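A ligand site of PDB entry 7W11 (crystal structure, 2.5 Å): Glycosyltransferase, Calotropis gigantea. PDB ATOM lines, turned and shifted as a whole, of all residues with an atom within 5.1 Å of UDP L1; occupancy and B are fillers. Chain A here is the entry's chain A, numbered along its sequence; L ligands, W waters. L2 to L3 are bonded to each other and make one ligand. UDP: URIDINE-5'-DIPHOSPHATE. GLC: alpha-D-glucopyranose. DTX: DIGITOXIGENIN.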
ATOM      1  N   GLU A  24      17.148  29.604   9.147  1.00  0.00           N
ATOM      2  CA  GLU A  24      18.133  28.549   9.261  1.00  0.00           C
ATOM      3  C   GLU A  24      19.503  29.194   9.054  1.00  0.00           C
ATOM      4  O   GLU A  24      19.641  30.049   8.173  1.00  0.00           O
ATOM      5  CB  GLU A  24      17.887  27.423   8.241  1.00  0.00           C
ATOM      6  CG  GLU A  24      18.752  26.188   8.441  1.00  0.00           C
ATOM      7  CD  GLU A  24      20.050  26.181   7.606  1.00  0.00           C
ATOM      8  OE1 GLU A  24      20.275  27.088   6.754  1.00  0.00           O
ATOM      9  OE2 GLU A  24      20.862  25.245   7.822  1.00  0.00           O
ATOM     10  N   LYS A  25      20.498  28.783   9.851  1.00  0.00           N
ATOM     11  CA  LYS A  25      21.717  29.566  10.008  1.00  0.00           C
ATOM     12  C   LYS A  25      22.455  29.763   8.691  1.00  0.00           C
ATOM     13  O   LYS A  25      23.020  30.841   8.450  1.00  0.00           O
ATOM     14  CB  LYS A  25      22.640  28.916  11.040  1.00  0.00           C
ATOM     15  CG  LYS A  25      22.828  29.714  12.283  1.00  0.00           C
ATOM     16  CD  LYS A  25      22.502  28.880  13.527  1.00  0.00           C
ATOM     17  CE  LYS A  25      22.127  29.790  14.693  1.00  0.00           C
ATOM     18  NZ  LYS A  25      21.503  29.042  15.799  1.00  0.00           N
ATOM     19  N   GLY A  26      22.488  28.743   7.826  1.00  0.00           N
ATOM     20  CA  GLY A  26      23.062  28.914   6.497  1.00  0.00           C
ATOM     21  C   GLY A  26      22.257  29.804   5.557  1.00  0.00           C
ATOM     22  O   GLY A  26      22.724  30.101   4.450  1.00  0.00           O
ATOM     23  N   ASN A  29      22.779  33.627   8.086  1.00  0.00           N
ATOM     24  CA  ASN A  29      24.116  34.205   8.165  1.00  0.00           C
ATOM     25  C   ASN A  29      24.474  35.055   6.946  1.00  0.00           C
ATOM     26  O   ASN A  29      24.965  36.176   7.128  1.00  0.00           O
ATOM     27  CB  ASN A  29      25.158  33.097   8.366  1.00  0.00           C
ATOM     28  CG  ASN A  29      25.320  32.704   9.844  1.00  0.00           C
ATOM     29  OD1 ASN A  29      24.722  33.327  10.724  1.00  0.00           O
ATOM     30  ND2 ASN A  29      26.133  31.653  10.104  1.00  0.00           N
ATOM     31  N   GLU A 261      29.230  35.507  17.826  1.00  0.00           N
ATOM     32  CA  GLU A 261      29.004  34.057  17.875  1.00  0.00           C
ATOM     33  C   GLU A 261      29.251  33.472  19.270  1.00  0.00           C
ATOM     34  O   GLU A 261      30.156  33.912  19.982  1.00  0.00           O
ATOM     35  CB  GLU A 261      29.897  33.348  16.863  1.00  0.00           C
ATOM     36  CG  GLU A 261      29.223  32.172  16.191  1.00  0.00           C
ATOM     37  CD  GLU A 261      27.759  32.432  15.927  1.00  0.00           C
ATOM     38  OE1 GLU A 261      27.460  33.443  15.255  1.00  0.00           O
ATOM     39  OE2 GLU A 261      26.920  31.660  16.402  1.00  0.00           O
ATOM     40  N   TYR A 281      40.113  21.572  12.268  1.00  0.00           N
ATOM     41  CA  TYR A 281      38.796  22.096  12.608  1.00  0.00           C
ATOM     42  C   TYR A 281      37.705  21.231  11.990  1.00  0.00           C
ATOM     43  O   TYR A 281      37.715  20.986  10.779  1.00  0.00           O
ATOM     44  CB  TYR A 281      38.650  23.549  12.139  1.00  0.00           C
ATOM     45  CG  TYR A 281      37.262  24.085  12.365  1.00  0.00           C
ATOM     46  CD1 TYR A 281      36.683  24.044  13.621  1.00  0.00           C
ATOM     47  CD2 TYR A 281      36.517  24.613  11.307  1.00  0.00           C
ATOM     48  CE1 TYR A 281      35.385  24.522  13.846  1.00  0.00           C
ATOM     49  CE2 TYR A 281      35.231  25.108  11.518  1.00  0.00           C
ATOM     50  CZ  TYR A 281      34.659  25.055  12.794  1.00  0.00           C
ATOM     51  OH  TYR A 281      33.378  25.519  13.009  1.00  0.00           O
ATOM     52  N   SER A 283      33.528  20.505  11.716  1.00  0.00           N
ATOM     53  CA  SER A 283      32.164  20.987  11.879  1.00  0.00           C
ATOM     54  C   SER A 283      31.299  20.439  10.759  1.00  0.00           C
ATOM     55  O   SER A 283      31.696  20.418   9.594  1.00  0.00           O
ATOM     56  CB  SER A 283      32.106  22.512  11.877  1.00  0.00           C
ATOM     57  OG  SER A 283      30.793  22.956  12.196  1.00  0.00           O
ATOM     58  N   GLY A 285      28.096  21.670  10.355  1.00  0.00           N
ATOM     59  CA  GLY A 285      27.035  22.640  10.174  1.00  0.00           C
ATOM     60  C   GLY A 285      26.073  22.662  11.337  1.00  0.00           C
ATOM     61  O   GLY A 285      26.366  22.281  12.468  1.00  0.00           O
ATOM     62  N   SER A 286      24.868  23.137  11.026  1.00  0.00           N
ATOM     63  CA  SER A 286      23.861  23.464  12.026  1.00  0.00           C
ATOM     64  C   SER A 286      22.650  22.548  11.964  1.00  0.00           C
ATOM     65  O   SER A 286      21.764  22.664  12.820  1.00  0.00           O
ATOM     66  CB  SER A 286      23.390  24.913  11.829  1.00  0.00           C
ATOM     67  OG  SER A 286      22.515  24.997  10.725  1.00  0.00           O
ATOM     68  N   ILE A 287      22.588  21.652  10.977  1.00  0.00           N
ATOM     69  CA  ILE A 287      21.466  20.746  10.781  1.00  0.00           C
ATOM     70  C   ILE A 287      21.931  19.292  10.781  1.00  0.00           C
ATOM     71  O   ILE A 287      21.379  18.451  11.503  1.00  0.00           O
ATOM     72  CB  ILE A 287      20.715  21.066   9.478  1.00  0.00           C
ATOM     73  CG1 ILE A 287      20.370  22.564   9.386  1.00  0.00           C
ATOM     74  CG2 ILE A 287      19.483  20.182   9.332  1.00  0.00           C
ATOM     75  CD1 ILE A 287      18.996  22.942   9.948  1.00  0.00           C
ATOM     76  N   VAL A 312      33.284  20.820  16.562  1.00  0.00           N
ATOM     77  CA  VAL A 312      31.981  21.313  16.973  1.00  0.00           C
ATOM     78  C   VAL A 312      31.021  20.133  17.016  1.00  0.00           C
ATOM     79  O   VAL A 312      30.844  19.415  16.025  1.00  0.00           O
ATOM     80  CB  VAL A 312      31.462  22.416  16.037  1.00  0.00           C
ATOM     81  CG1 VAL A 312      30.046  22.815  16.431  1.00  0.00           C
ATOM     82  CG2 VAL A 312      32.375  23.630  16.076  1.00  0.00           C
ATOM     83  N   TRP A 353      29.432  25.006  19.881  1.00  0.00           N
ATOM     84  CA  TRP A 353      29.312  26.071  18.888  1.00  0.00           C
ATOM     85  C   TRP A 353      30.512  27.001  18.972  1.00  0.00           C
ATOM     86  O   TRP A 353      31.046  27.231  20.068  1.00  0.00           O
ATOM     87  CB  TRP A 353      28.016  26.852  19.092  1.00  0.00           C
ATOM     88  CG  TRP A 353      27.558  27.528  17.835  1.00  0.00           C
ATOM     89  CD1 TRP A 353      27.543  28.869  17.588  1.00  0.00           C
ATOM     90  CD2 TRP A 353      27.052  26.887  16.652  1.00  0.00           C
ATOM     91  NE1 TRP A 353      27.055  29.092  16.312  1.00  0.00           N
ATOM     92  CE2 TRP A 353      26.750  27.896  15.719  1.00  0.00           C
ATOM     93  CE3 TRP A 353      26.814  25.558  16.289  1.00  0.00           C
ATOM     94  CZ2 TRP A 353      26.236  27.628  14.467  1.00  0.00           C
ATOM     95  CZ3 TRP A 353      26.312  25.283  15.039  1.00  0.00           C
ATOM     96  CH2 TRP A 353      26.023  26.321  14.140  1.00  0.00           C
ATOM     97  N   CYS A 354      30.942  27.535  17.846  1.00  0.00           N
ATOM     98  CA  CYS A 354      32.134  28.376  17.828  1.00  0.00           C
ATOM     99  C   CYS A 354      31.913  29.524  16.850  1.00  0.00           C
ATOM    100  O   CYS A 354      30.944  29.503  16.077  1.00  0.00           O
ATOM    101  CB  CYS A 354      33.358  27.548  17.428  1.00  0.00           C
ATOM    102  SG  CYS A 354      33.485  27.166  15.638  1.00  0.00           S
ATOM    103  N   PRO A 355      32.768  30.543  16.871  1.00  0.00           N
ATOM    104  CA  PRO A 355      32.740  31.537  15.787  1.00  0.00           C
ATOM    105  C   PRO A 355      33.482  30.992  14.572  1.00  0.00           C
ATOM    106  O   PRO A 355      34.699  31.144  14.472  1.00  0.00           O
ATOM    107  CB  PRO A 355      33.445  32.753  16.404  1.00  0.00           C
ATOM    108  CG  PRO A 355      34.407  32.139  17.425  1.00  0.00           C
ATOM    109  CD  PRO A 355      33.853  30.794  17.841  1.00  0.00           C
ATOM    110  N   GLN A 356      32.763  30.340  13.659  1.00  0.00           N
ATOM    111  CA  GLN A 356      33.447  29.533  12.655  1.00  0.00           C
ATOM    112  C   GLN A 356      34.380  30.370  11.782  1.00  0.00           C
ATOM    113  O   GLN A 356      35.515  29.975  11.534  1.00  0.00           O
ATOM    114  CB  GLN A 356      32.422  28.798  11.802  1.00  0.00           C
ATOM    115  CG  GLN A 356      33.002  28.363  10.485  1.00  0.00           C
ATOM    116  CD  GLN A 356      32.231  27.232   9.873  1.00  0.00           C
ATOM    117  OE1 GLN A 356      31.689  27.360   8.781  1.00  0.00           O
ATOM    118  NE2 GLN A 356      32.205  26.099  10.557  1.00  0.00           N
ATOM    119  N   LEU A 357      33.917  31.534  11.322  1.00  0.00           N
ATOM    120  CA  LEU A 357      34.725  32.375  10.458  1.00  0.00           C
ATOM    121  C   LEU A 357      36.055  32.733  11.098  1.00  0.00           C
ATOM    122  O   LEU A 357      37.104  32.757  10.426  1.00  0.00           O
ATOM    123  CB  LEU A 357      33.966  33.643  10.093  1.00  0.00           C
ATOM    124  CG  LEU A 357      34.684  34.457   9.012  1.00  0.00           C
ATOM    125  CD1 LEU A 357      35.306  33.517   7.995  1.00  0.00           C
ATOM    126  CD2 LEU A 357      33.719  35.436   8.343  1.00  0.00           C
ATOM    127  N   HIS A 371      31.100  19.311   6.341  1.00  0.00           N
ATOM    128  CA  HIS A 371      30.005  18.715   5.593  1.00  0.00           C
ATOM    129  C   HIS A 371      29.776  19.411   4.258  1.00  0.00           C
ATOM    130  O   HIS A 371      28.932  18.961   3.474  1.00  0.00           O
ATOM    131  CB  HIS A 371      28.750  18.717   6.461  1.00  0.00           C
ATOM    132  CG  HIS A 371      28.021  20.014   6.480  1.00  0.00           C
ATOM    133  ND1 HIS A 371      28.595  21.185   6.917  1.00  0.00           N
ATOM    134  CD2 HIS A 371      26.755  20.334   6.107  1.00  0.00           C
ATOM    135  CE1 HIS A 371      27.716  22.171   6.825  1.00  0.00           C
ATOM    136  NE2 HIS A 371      26.592  21.687   6.328  1.00  0.00           N
ATOM    137  N   GLY A 373      28.432  22.392   3.479  1.00  0.00           N
ATOM    138  CA  GLY A 373      27.430  23.423   3.245  1.00  0.00           C
ATOM    139  C   GLY A 373      28.088  24.603   2.586  1.00  0.00           C
ATOM    140  O   GLY A 373      29.291  24.821   2.727  1.00  0.00           O
ATOM    141  N   TRP A 374      27.297  25.382   1.802  1.00  0.00           N
ATOM    142  CA  TRP A 374      27.949  26.393   0.963  1.00  0.00           C
ATOM    143  C   TRP A 374      28.532  27.531   1.792  1.00  0.00           C
ATOM    144  O   TRP A 374      29.592  28.073   1.423  1.00  0.00           O
ATOM    145  CB  TRP A 374      26.997  26.964  -0.089  1.00  0.00           C
ATOM    146  CG  TRP A 374      27.671  28.043  -0.913  1.00  0.00           C
ATOM    147  CD1 TRP A 374      27.325  29.354  -0.973  1.00  0.00           C
ATOM    148  CD2 TRP A 374      28.825  27.890  -1.767  1.00  0.00           C
ATOM    149  NE1 TRP A 374      28.179  30.042  -1.803  1.00  0.00           N
ATOM    150  CE2 TRP A 374      29.112  29.167  -2.301  1.00  0.00           C
ATOM    151  CE3 TRP A 374      29.650  26.813  -2.106  1.00  0.00           C
ATOM    152  CZ2 TRP A 374      30.187  29.389  -3.178  1.00  0.00           C
ATOM    153  CZ3 TRP A 374      30.726  27.035  -2.983  1.00  0.00           C
ATOM    154  CH2 TRP A 374      30.983  28.322  -3.501  1.00  0.00           C
ATOM    155  N   ASN A 375      27.901  27.897   2.901  1.00  0.00           N
ATOM    156  CA  ASN A 375      28.507  28.923   3.738  1.00  0.00           C
ATOM    157  C   ASN A 375      29.851  28.452   4.295  1.00  0.00           C
ATOM    158  O   ASN A 375      30.860  29.168   4.199  1.00  0.00           O
ATOM    159  CB  ASN A 375      27.557  29.328   4.863  1.00  0.00           C
ATOM    160  CG  ASN A 375      26.329  30.015   4.358  1.00  0.00           C
ATOM    161  OD1 ASN A 375      26.346  31.207   4.056  1.00  0.00           O
ATOM    162  ND2 ASN A 375      25.233  29.268   4.258  1.00  0.00           N
ATOM    163  N   SER A 376      29.892  27.245   4.869  1.00  0.00           N
ATOM    164  CA  SER A 376      31.157  26.681   5.344  1.00  0.00           C
ATOM    165  C   SER A 376      32.198  26.633   4.218  1.00  0.00           C
ATOM    166  O   SER A 376      33.369  26.988   4.422  1.00  0.00           O
ATOM    167  CB  SER A 376      30.918  25.284   5.912  1.00  0.00           C
ATOM    168  OG  SER A 376      30.286  25.376   7.170  1.00  0.00           O
ATOM    169  N   THR A 377      31.793  26.173   3.030  1.00  0.00           N
ATOM    170  CA  THR A 377      32.744  26.075   1.917  1.00  0.00           C
ATOM    171  C   THR A 377      33.285  27.431   1.533  1.00  0.00           C
ATOM    172  O   THR A 377      34.500  27.607   1.363  1.00  0.00           O
ATOM    173  CB  THR A 377      32.089  25.404   0.714  1.00  0.00           C
ATOM    174  OG1 THR A 377      31.576  24.121   1.095  1.00  0.00           O
ATOM    175  CG2 THR A 377      33.097  25.224  -0.384  1.00  0.00           C
ATOM    176  N   GLU A 379      33.261  30.234   3.386  1.00  0.00           N
ATOM    177  CA  GLU A 379      34.061  30.804   4.461  1.00  0.00           C
ATOM    178  C   GLU A 379      35.493  30.265   4.420  1.00  0.00           C
ATOM    179  O   GLU A 379      36.451  31.032   4.528  1.00  0.00           O
ATOM    180  CB  GLU A 379      33.402  30.538   5.814  1.00  0.00           C
ATOM    181  CG  GLU A 379      32.207  31.401   6.081  1.00  0.00           C
ATOM    182  CD  GLU A 379      31.201  30.772   7.024  1.00  0.00           C
ATOM    183  OE1 GLU A 379      31.601  29.919   7.857  1.00  0.00           O
ATOM    184  OE2 GLU A 379      30.007  31.131   6.942  1.00  0.00           O
ATOM    185  N   TRP A 393      24.055  16.103   2.333  1.00  0.00           N
ATOM    186  CA  TRP A 393      22.914  16.058   1.417  1.00  0.00           C
ATOM    187  C   TRP A 393      22.724  17.388   0.695  1.00  0.00           C
ATOM    188  O   TRP A 393      23.515  18.323   0.825  1.00  0.00           O
ATOM    189  CB  TRP A 393      21.641  15.622   2.165  1.00  0.00           C
ATOM    190  CG  TRP A 393      21.605  15.993   3.610  1.00  0.00           C
ATOM    191  CD1 TRP A 393      21.692  15.136   4.686  1.00  0.00           C
ATOM    192  CD2 TRP A 393      21.512  17.316   4.145  1.00  0.00           C
ATOM    193  NE1 TRP A 393      21.617  15.858   5.864  1.00  0.00           N
ATOM    194  CE2 TRP A 393      21.515  17.195   5.558  1.00  0.00           C
ATOM    195  CE3 TRP A 393      21.402  18.563   3.584  1.00  0.00           C
ATOM    196  CZ2 TRP A 393      21.428  18.299   6.399  1.00  0.00           C
ATOM    197  CZ3 TRP A 393      21.321  19.660   4.415  1.00  0.00           C
ATOM    198  CH2 TRP A 393      21.332  19.524   5.815  1.00  0.00           C
ATOM    199  N   GLN A 396      25.579  19.831  -0.640  1.00  0.00           N
ATOM    200  CA  GLN A 396      26.898  19.459  -0.137  1.00  0.00           C
ATOM    201  C   GLN A 396      27.644  18.508  -1.068  1.00  0.00           C
ATOM    202  O   GLN A 396      28.875  18.589  -1.162  1.00  0.00           O
ATOM    203  CB  GLN A 396      26.782  18.850   1.253  1.00  0.00           C
ATOM    204  CG  GLN A 396      26.425  19.863   2.303  1.00  0.00           C
ATOM    205  CD  GLN A 396      25.451  19.302   3.328  1.00  0.00           C
ATOM    206  OE1 GLN A 396      25.474  18.115   3.665  1.00  0.00           O
ATOM    207  NE2 GLN A 396      24.571  20.165   3.806  1.00  0.00           N
HETATM  208  N1  UDP L   1      28.601  27.939  12.046  1.00  0.00           N
HETATM  209  C2  UDP L   1      28.991  28.599  13.115  1.00  0.00           C
HETATM  210  N3  UDP L   1      29.497  28.020  14.175  1.00  0.00           N
HETATM  211  C4  UDP L   1      29.645  26.713  14.179  1.00  0.00           C
HETATM  212  C5  UDP L   1      29.266  25.970  13.069  1.00  0.00           C
HETATM  213  C6  UDP L   1      28.721  26.628  11.976  1.00  0.00           C
HETATM  214  O2  UDP L   1      28.811  29.972  13.099  1.00  0.00           O
HETATM  215  O4  UDP L   1      30.210  26.095  15.311  1.00  0.00           O
HETATM  216  C1' UDP L   1      28.045  28.756  10.942  1.00  0.00           C
HETATM  217  C2' UDP L   1      28.936  28.656   9.692  1.00  0.00           C
HETATM  218  O2' UDP L   1      29.988  29.543   9.765  1.00  0.00           O
HETATM  219  C3' UDP L   1      27.917  28.948   8.552  1.00  0.00           C
HETATM  220  C4' UDP L   1      26.769  28.465   8.977  1.00  0.00           C
HETATM  221  O4' UDP L   1      26.861  28.322  10.582  1.00  0.00           O
HETATM  222  O3' UDP L   1      27.767  30.421   8.293  1.00  0.00           O
HETATM  223  C5' UDP L   1      26.530  27.074   8.445  1.00  0.00           C
HETATM  224  O5' UDP L   1      26.014  27.236   7.165  1.00  0.00           O
HETATM  225  PA  UDP L   1      26.310  26.068   6.053  1.00  0.00           P
HETATM  226  O1A UDP L   1      27.799  25.845   6.010  1.00  0.00           O
HETATM  227  O2A UDP L   1      25.855  26.551   4.698  1.00  0.00           O
HETATM  228  O3A UDP L   1      25.601  24.624   6.416  1.00  0.00           O
HETATM  229  PB  UDP L   1      24.125  24.374   7.094  1.00  0.00           P
HETATM  230  O1B UDP L   1      23.765  22.929   6.814  1.00  0.00           O
HETATM  231  O2B UDP L   1      24.240  24.604   8.575  1.00  0.00           O
HETATM  232  O3B UDP L   1      23.034  25.240   6.485  1.00  0.00           O
HETATM  233  C1  GLC L   2      20.974  24.372   3.556  1.00  0.00           C
HETATM  234  C2  GLC L   2      21.955  23.260   3.414  1.00  0.00           C
HETATM  235  C3  GLC L   2      23.375  23.784   3.145  1.00  0.00           C
HETATM  236  C4  GLC L   2      23.331  24.911   2.169  1.00  0.00           C
HETATM  237  C5  GLC L   2      22.567  26.064   2.807  1.00  0.00           C
HETATM  238  C6  GLC L   2      21.963  26.975   1.747  1.00  0.00           C
HETATM  239  O2  GLC L   2      22.031  22.399   4.551  1.00  0.00           O
HETATM  240  O3  GLC L   2      24.165  22.712   2.624  1.00  0.00           O
HETATM  241  O4  GLC L   2      24.615  25.400   1.818  1.00  0.00           O
HETATM  242  O5  GLC L   2      21.545  25.649   3.720  1.00  0.00           O
HETATM  243  O6  GLC L   2      22.332  28.316   1.979  1.00  0.00           O
HETATM  244  O23 DTX L   3      10.411  17.855  10.388  1.00  0.00           O
HETATM  245  C23 DTX L   3      10.750  18.991  10.163  1.00  0.00           C
HETATM  246  C22 DTX L   3      12.072  19.574   9.979  1.00  0.00           C
HETATM  247  O21 DTX L   3       9.822  19.958  10.041  1.00  0.00           O
HETATM  248  C21 DTX L   3      10.493  21.211   9.784  1.00  0.00           C
HETATM  249  C20 DTX L   3      11.934  20.846   9.633  1.00  0.00           C
HETATM  250  C17 DTX L   3      12.974  21.828   9.157  1.00  0.00           C
HETATM  251  C16 DTX L   3      14.346  21.676   9.857  1.00  0.00           C
HETATM  252  C13 DTX L   3      13.267  21.783   7.631  1.00  0.00           C
HETATM  253  C12 DTX L   3      13.574  23.219   7.181  1.00  0.00           C
HETATM  254  C11 DTX L   3      14.181  23.265   5.783  1.00  0.00           C
HETATM  255  C18 DTX L   3      12.132  21.214   6.794  1.00  0.00           C
HETATM  256  C14 DTX L   3      14.572  20.929   7.539  1.00  0.00           C
HETATM  257  C15 DTX L   3      15.380  21.400   8.750  1.00  0.00           C
HETATM  258  O14 DTX L   3      14.215  19.544   7.763  1.00  0.00           O
HETATM  259  C8  DTX L   3      15.271  21.027   6.182  1.00  0.00           C
HETATM  260  C7  DTX L   3      16.606  20.268   6.190  1.00  0.00           C
HETATM  261  C9  DTX L   3      15.492  22.478   5.690  1.00  0.00           C
HETATM  262  C10 DTX L   3      16.181  22.548   4.290  1.00  0.00           C
HETATM  263  C1  DTX L   3      16.496  24.009   3.892  1.00  0.00           C
HETATM  264  C19 DTX L   3      15.283  21.964   3.193  1.00  0.00           C
HETATM  265  C5  DTX L   3      17.521  21.763   4.389  1.00  0.00           C
HETATM  266  C6  DTX L   3      17.295  20.321   4.829  1.00  0.00           C
HETATM  267  C4  DTX L   3      18.566  22.490   5.256  1.00  0.00           C
HETATM  268  C3  DTX L   3      18.795  23.953   4.823  1.00  0.00           C
HETATM  269  C2  DTX L   3      17.978  24.247   3.602  1.00  0.00           C
HETATM  270  O32 DTX L   3      20.224  24.126   4.726  1.00  0.00           O
HETATM  271  O   HOH W   1      26.184  31.032  12.986  1.00  0.00           O
HETATM  272  O   HOH W   2      29.029  33.425   9.485  1.00  0.00           O
HETATM  273  O   HOH W   3      23.978  20.938   8.757  1.00  0.00           O
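An oxygen (O2') of UDP L1 lies within hydrogen-bond range of the side-chain carboxylate (OE1) of Glu 379, at 2.5 Å.
An oxygen (O3B) of UDP L1 sits close to the side-chain carboxylate (OE2) of Glu 24 (2.6 Å).
ND2 of Asn 29 sits at hydrogen-bond distance from O3' of UDP L1, at 2.7 Å.
An oxygen (O1A) of UDP L1 is in hydrogen-bond range of the backbone NH (N) of Ser 376 (2.8 Å).
The side-chain hydroxyl of Ser 376 sits at hydrogen-bond distance from an oxygen (O1A) of UDP L1, at 2.8 Å.
N of Ser 286 sits at hydrogen-bond distance from O2B of UDP L1 (2.9 Å).
The side-chain hydroxyl of Ser 286 sits at hydrogen-bond distance from an oxygen (O2B) of UDP L1, 2.8 Å away.
N of Cys 354 is in hydrogen-bond range of O4 of UDP L1, at 3.0 Å.
The backbone carbonyl oxygen of Cys 354 sits at hydrogen-bond distance from a nitrogen (N3) of UDP L1 (2.8 Å).
The side-chain sulfur (SG) of Cys 354 is in hydrogen-bond range of an oxygen (O4) of UDP L1 (3.5 Å).
The backbone NH (N) of Asn 375 is in hydrogen-bond range of an oxygen (O2A) of UDP L1 (3.0 Å).
The side-chain amide nitrogen (ND2) of Asn 375 is in hydrogen-bond range of an oxygen (O2A) of UDP L1 (2.8 Å).
O2' of UDP L1 lies within hydrogen-bond range of OE1 of Gln 356, 2.9 Å away.
NE2 of His 371 lies within hydrogen-bond range of O3A of UDP L1.
The backbone NH (N) of Trp 374 lies within hydrogen-bond range of an oxygen (O2A) of UDP L1.
The backbone NH (N) of Trp 374 is in hydrogen-bond range of an oxygen (O4) of GLC L2 (2.7 Å).
The backbone carbonyl oxygen (O) of Gly 26 sits at hydrogen-bond distance from an oxygen (O6) of GLC L2.
NE2 of Gln 396 lies within hydrogen-bond range of O3 of GLC L2.
An oxygen (O1B) of UDP L1 sits at hydrogen-bond distance from an oxygen (O2) of GLC L2, 2.9 Å away.
The side-chain carboxylate of Glu 379 lies close to the side-chain amide oxygen of Gln 356 (2.7 Å).
OE2 of Glu 24 is in hydrogen-bond range of OG of Ser 286, at 3.3 Å.
OE1 of Glu 24 lies within hydrogen-bond range of N of Gly 26 (3.0 Å).
The side-chain sulfur (SG) of Cys 354 sits at hydrogen-bond distance from the side-chain hydroxyl (OH) of Tyr 281, at 3.1 Å.
The side-chain amide nitrogen of Asn 375 sits at hydrogen-bond distance from the backbone carbonyl oxygen of Gly 26 (2.7 Å).
NE2 of Gln 356 lies within hydrogen-bond range of OH of Tyr 281 (2.8 Å).
O of Ser 283 lies within hydrogen-bond range of N of His 371 (3.5 Å).
A ring nitrogen (NE2) of His 371 sits close to the backbone NH (N) of Gly 373, 3.5 Å away.
The indole nitrogen of Trp 353 sits close to a nitrogen (N3) of UDP L1, 3.4 Å away.
Residues that only touch UDP L1: Gly 26 (3.5 Å), Glu 261 (3.8 Å), Tyr 281 (3.96 Å), Ser 283 (3.5 Å), Gly 285 (3.8 Å), Val 312 (3.4 Å) and Gly 373 (3.6 Å).
Hydrophobic or aromatic side chains within 4 Å of UDP L1: Val 312, Trp 353 and His 371.
Within 4 Å of UDP L1: Glu 24, Gly 26, Asn 29, Glu 261, Tyr 281, Ser 283, Gly 285, Ser 286, Val 312, Trp 353, Cys 354, Gln 356, His 371, Gly 373, Trp 374, Asn 375, Ser 376 and Glu 379.
The nearest printed residue that does not touch UDP L1 is Ile 287 (4.1 Å).
Water W3 lies within hydrogen-bond range of the backbone NH of Ile 287 (2.7 Å), an oxygen (O1B) of UDP L1 (2.8 Å) and the backbone NH of Ser 286 (3.3 Å).
Water W1 lies within hydrogen-bond range of an oxygen (O2) of UDP L1 and the side-chain amide nitrogen (ND2) of Asn 29.
Water W2 lies within hydrogen-bond range of the side-chain amide nitrogen (ND2) of Asn 29 (3.5 Å) and an oxygen (O3') of UDP L1 (3.5 Å).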
